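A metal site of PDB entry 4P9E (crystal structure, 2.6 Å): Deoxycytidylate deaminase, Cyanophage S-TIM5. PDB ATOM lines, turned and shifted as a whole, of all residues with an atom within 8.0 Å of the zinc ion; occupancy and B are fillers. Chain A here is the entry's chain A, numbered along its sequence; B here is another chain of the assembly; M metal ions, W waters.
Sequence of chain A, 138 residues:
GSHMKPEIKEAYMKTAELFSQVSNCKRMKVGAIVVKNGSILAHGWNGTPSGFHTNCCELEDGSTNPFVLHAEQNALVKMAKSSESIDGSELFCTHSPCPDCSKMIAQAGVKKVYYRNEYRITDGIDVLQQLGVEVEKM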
ATOM      1  N   VAL A  30      -6.581  -1.562   8.671  1.00  0.00           N
ATOM      2  CA  VAL A  30      -7.728  -0.723   8.329  1.00  0.00           C
ATOM      3  C   VAL A  30      -8.179  -0.972   6.889  1.00  0.00           C
ATOM      4  O   VAL A  30      -7.350  -1.174   5.986  1.00  0.00           O
ATOM      5  CB  VAL A  30      -7.363   0.774   8.466  1.00  0.00           C
ATOM      6  CG1 VAL A  30      -8.612   1.654   8.413  1.00  0.00           C
ATOM      7  CG2 VAL A  30      -6.597   1.015   9.760  1.00  0.00           C
ATOM      8  N   LEU A  69       0.539   4.553   3.679  1.00  0.00           N
ATOM      9  CA  LEU A  69      -0.712   5.268   3.448  1.00  0.00           C
ATOM     10  C   LEU A  69      -1.821   4.652   4.287  1.00  0.00           C
ATOM     11  O   LEU A  69      -1.864   3.440   4.478  1.00  0.00           O
ATOM     12  CB  LEU A  69      -1.104   5.169   1.977  1.00  0.00           C
ATOM     13  CG  LEU A  69       0.022   5.552   1.021  1.00  0.00           C
ATOM     14  CD1 LEU A  69       0.288   4.424   0.028  1.00  0.00           C
ATOM     15  CD2 LEU A  69      -0.321   6.832   0.326  1.00  0.00           C
ATOM     16  N   HIS A  70      -2.719   5.496   4.781  1.00  0.00           N
ATOM     17  CA  HIS A  70      -3.904   5.024   5.463  1.00  0.00           C
ATOM     18  C   HIS A  70      -4.857   4.492   4.406  1.00  0.00           C
ATOM     19  O   HIS A  70      -4.754   4.841   3.236  1.00  0.00           O
ATOM     20  CB  HIS A  70      -4.541   6.149   6.249  1.00  0.00           C
ATOM     21  CG  HIS A  70      -3.670   6.674   7.351  1.00  0.00           C
ATOM     22  ND1 HIS A  70      -4.009   7.780   8.092  1.00  0.00           N
ATOM     23  CD2 HIS A  70      -2.494   6.237   7.825  1.00  0.00           C
ATOM     24  CE1 HIS A  70      -3.059   8.011   8.977  1.00  0.00           C
ATOM     25  NE2 HIS A  70      -2.130   7.088   8.843  1.00  0.00           N
ATOM     26  N   ALA A  71      -5.776   3.639   4.837  1.00  0.00           N
ATOM     27  CA  ALA A  71      -6.772   3.052   3.950  1.00  0.00           C
ATOM     28  C   ALA A  71      -7.545   4.126   3.184  1.00  0.00           C
ATOM     29  O   ALA A  71      -7.865   3.960   2.016  1.00  0.00           O
ATOM     30  CB  ALA A  71      -7.723   2.188   4.762  1.00  0.00           C
ATOM     31  N   GLU A  72      -7.836   5.232   3.871  1.00  0.00           N
ATOM     32  CA  GLU A  72      -8.616   6.309   3.305  1.00  0.00           C
ATOM     33  C   GLU A  72      -7.795   7.036   2.237  1.00  0.00           C
ATOM     34  O   GLU A  72      -8.316   7.377   1.181  1.00  0.00           O
ATOM     35  CB  GLU A  72      -9.090   7.285   4.389  1.00  0.00           C
ATOM     36  CG  GLU A  72      -9.871   6.678   5.565  1.00  0.00           C
ATOM     37  CD  GLU A  72      -8.975   6.196   6.712  1.00  0.00           C
ATOM     38  OE1 GLU A  72      -7.894   5.619   6.451  1.00  0.00           O
ATOM     39  OE2 GLU A  72      -9.375   6.384   7.878  1.00  0.00           O
ATOM     40  N   GLN A  73      -6.519   7.271   2.510  1.00  0.00           N
ATOM     41  CA  GLN A  73      -5.592   7.762   1.495  1.00  0.00           C
ATOM     42  C   GLN A  73      -5.524   6.901   0.221  1.00  0.00           C
ATOM     43  O   GLN A  73      -5.521   7.422  -0.897  1.00  0.00           O
ATOM     44  CB  GLN A  73      -4.220   7.962   2.103  1.00  0.00           C
ATOM     45  CG  GLN A  73      -4.150   9.200   2.954  1.00  0.00           C
ATOM     46  CD  GLN A  73      -2.992   9.227   3.928  1.00  0.00           C
ATOM     47  OE1 GLN A  73      -2.129   8.347   3.932  1.00  0.00           O
ATOM     48  NE2 GLN A  73      -2.970  10.242   4.796  1.00  0.00           N
ATOM     49  N   CYS A  93     -15.433   2.864   6.522  1.00  0.00           N
ATOM     50  CA  CYS A  93     -14.125   2.501   6.992  1.00  0.00           C
ATOM     51  C   CYS A  93     -14.230   1.599   8.248  1.00  0.00           C
ATOM     52  O   CYS A  93     -15.188   1.699   9.002  1.00  0.00           O
ATOM     53  CB  CYS A  93     -13.305   3.769   7.250  1.00  0.00           C
ATOM     54  SG  CYS A  93     -11.514   3.469   7.356  1.00  0.00           S
ATOM     55  N   HIS A  95     -12.186   1.905  10.646  1.00  0.00           N
ATOM     56  CA  HIS A  95     -11.838   2.804  11.724  1.00  0.00           C
ATOM     57  C   HIS A  95     -12.242   4.233  11.486  1.00  0.00           C
ATOM     58  O   HIS A  95     -12.283   4.679  10.347  1.00  0.00           O
ATOM     59  CB  HIS A  95     -10.348   2.734  12.016  1.00  0.00           C
ATOM     60  CG  HIS A  95      -9.908   1.407  12.540  1.00  0.00           C
ATOM     61  ND1 HIS A  95      -9.854   0.279  11.748  1.00  0.00           N
ATOM     62  CD2 HIS A  95      -9.531   1.027  13.776  1.00  0.00           C
ATOM     63  CE1 HIS A  95      -9.436  -0.738  12.482  1.00  0.00           C
ATOM     64  NE2 HIS A  95      -9.228  -0.319  13.711  1.00  0.00           N
ATOM     65  N   SER A  96     -12.561   4.933  12.572  1.00  0.00           N
ATOM     66  CA  SER A  96     -12.645   6.376  12.603  1.00  0.00           C
ATOM     67  C   SER A  96     -11.368   6.924  11.960  1.00  0.00           C
ATOM     68  O   SER A  96     -10.295   6.376  12.176  1.00  0.00           O
ATOM     69  CB  SER A  96     -12.798   6.837  14.068  1.00  0.00           C
ATOM     70  OG  SER A  96     -12.129   8.054  14.365  1.00  0.00           O
ATOM     71  N   PRO A  97     -11.476   7.963  11.110  1.00  0.00           N
ATOM     72  CA  PRO A  97     -10.274   8.485  10.451  1.00  0.00           C
ATOM     73  C   PRO A  97      -9.463   9.500  11.259  1.00  0.00           C
ATOM     74  O   PRO A  97      -9.997  10.234  12.073  1.00  0.00           O
ATOM     75  CB  PRO A  97     -10.817   9.135   9.178  1.00  0.00           C
ATOM     76  CG  PRO A  97     -12.197   9.466   9.490  1.00  0.00           C
ATOM     77  CD  PRO A  97     -12.693   8.404  10.412  1.00  0.00           C
ATOM     78  N   CYS A  98      -8.156   9.513  11.002  1.00  0.00           N
ATOM     79  CA  CYS A  98      -7.235  10.454  11.618  1.00  0.00           C
ATOM     80  C   CYS A  98      -7.544  11.870  11.145  1.00  0.00           C
ATOM     81  O   CYS A  98      -8.327  12.046  10.236  1.00  0.00           O
ATOM     82  CB  CYS A  98      -5.786  10.061  11.289  1.00  0.00           C
ATOM     83  SG  CYS A  98      -5.195  10.494   9.622  1.00  0.00           S
ATOM     84  N   PRO A  99      -6.935  12.892  11.782  1.00  0.00           N
ATOM     85  CA  PRO A  99      -7.169  14.250  11.299  1.00  0.00           C
ATOM     86  C   PRO A  99      -6.733  14.502   9.852  1.00  0.00           C
ATOM     87  O   PRO A  99      -7.408  15.276   9.175  1.00  0.00           O
ATOM     88  CB  PRO A  99      -6.351  15.103  12.272  1.00  0.00           C
ATOM     89  CG  PRO A  99      -6.348  14.327  13.518  1.00  0.00           C
ATOM     90  CD  PRO A  99      -6.222  12.895  13.077  1.00  0.00           C
ATOM     91  N   ASP A 100      -5.650  13.877   9.388  1.00  0.00           N
ATOM     92  CA  ASP A 100      -5.137  14.090   8.034  1.00  0.00           C
ATOM     93  C   ASP A 100      -6.072  13.515   6.963  1.00  0.00           C
ATOM     94  O   ASP A 100      -6.222  14.064   5.864  1.00  0.00           O
ATOM     95  CB  ASP A 100      -3.736  13.499   7.858  1.00  0.00           C
ATOM     96  CG  ASP A 100      -2.739  14.006   8.907  1.00  0.00           C
ATOM     97  OD1 ASP A 100      -2.865  15.188   9.339  1.00  0.00           O
ATOM     98  OD2 ASP A 100      -1.820  13.221   9.290  1.00  0.00           O
ATOM     99  N   CYS A 101      -6.686  12.380   7.271  1.00  0.00           N
ATOM    100  CA  CYS A 101      -7.646  11.812   6.361  1.00  0.00           C
ATOM    101  C   CYS A 101      -8.931  12.618   6.417  1.00  0.00           C
ATOM    102  O   CYS A 101      -9.538  12.913   5.395  1.00  0.00           O
ATOM    103  CB  CYS A 101      -7.873  10.333   6.673  1.00  0.00           C
ATOM    104  SG  CYS A 101      -6.400   9.300   6.359  1.00  0.00           S
ATOM    105  N   SER A 102      -9.332  13.036   7.614  1.00  0.00           N
ATOM    106  CA  SER A 102     -10.514  13.863   7.766  1.00  0.00           C
ATOM    107  C   SER A 102     -10.552  15.156   6.933  1.00  0.00           C
ATOM    108  O   SER A 102     -11.570  15.452   6.312  1.00  0.00           O
ATOM    109  CB  SER A 102     -10.718  14.192   9.237  1.00  0.00           C
ATOM    110  OG  SER A 102     -11.030  13.006   9.947  1.00  0.00           O
ATOM    111  N   MET A 104      -9.204  15.678   4.166  1.00  0.00           N
ATOM    112  CA  MET A 104      -9.242  15.365   2.755  1.00  0.00           C
ATOM    113  C   MET A 104     -10.605  14.839   2.359  1.00  0.00           C
ATOM    114  O   MET A 104     -11.157  15.205   1.312  1.00  0.00           O
ATOM    115  CB  MET A 104      -8.152  14.363   2.410  1.00  0.00           C
ATOM    116  CG  MET A 104      -6.754  14.927   2.592  1.00  0.00           C
ATOM    117  SD  MET A 104      -5.514  14.016   1.641  1.00  0.00           S
ATOM    118  CE  MET A 104      -5.137  12.690   2.783  1.00  0.00           C
ATOM    119  N   ILE A 105     -11.135  13.982   3.229  1.00  0.00           N
ATOM    120  CA  ILE A 105     -12.478  13.477   3.108  1.00  0.00           C
ATOM    121  C   ILE A 105     -13.480  14.638   3.010  1.00  0.00           C
ATOM    122  O   ILE A 105     -14.374  14.622   2.157  1.00  0.00           O
ATOM    123  CB  ILE A 105     -12.782  12.570   4.307  1.00  0.00           C
ATOM    124  CG1 ILE A 105     -11.864  11.359   4.281  1.00  0.00           C
ATOM    125  CG2 ILE A 105     -14.227  12.118   4.319  1.00  0.00           C
ATOM    126  CD1 ILE A 105     -11.790  10.624   5.587  1.00  0.00           C
ATOM    127  N   LYS B 103       4.070  10.237  -0.731  1.00  0.00           N
ATOM    128  CA  LYS B 103       3.449   8.915  -0.751  1.00  0.00           C
ATOM    129  C   LYS B 103       2.284   8.876  -1.724  1.00  0.00           C
ATOM    130  O   LYS B 103       2.064   7.889  -2.418  1.00  0.00           O
ATOM    131  CB  LYS B 103       2.814   8.582   0.605  1.00  0.00           C
ATOM    132  CG  LYS B 103       3.695   8.540   1.808  1.00  0.00           C
ATOM    133  CD  LYS B 103       2.879   8.188   3.065  1.00  0.00           C
ATOM    134  CE  LYS B 103       1.716   9.129   3.317  1.00  0.00           C
ATOM    135  NZ  LYS B 103       1.287   9.104   4.736  1.00  0.00           N
HETATM  136 ZN    ZN M   1      -5.704   8.713   8.463  1.00  0.00          ZN
HETATM  137  O   HOH W   1      -7.264   6.995   9.257  1.00  0.00           O
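The backbone carbonyl oxygen (O) of Cys 98 lies within hydrogen-bond range of the side-chain hydroxyl (OG) of Ser 102 (2.9 Å).
SG of Cys 98 lies close to N of Asp 100, at 3.4 Å.
The side-chain amide oxygen (OE1) of Gln 73 lies within hydrogen-bond range of the backbone NH (N) of His 70 (3.0 Å).
ND1 of His 70 binds the zinc ion, at 2.0 Å.
The side-chain sulfur (SG) of Cys 98 binds the zinc ion.
The side-chain sulfur (SG) of Cys 101 binds the zinc ion (2.3 Å).
The zinc ion is bound by water W1.
Water W1 bridges the side-chain carboxylate of Glu 72 (2.6 Å) and the backbone NH of Cys 98 (3.2 Å).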
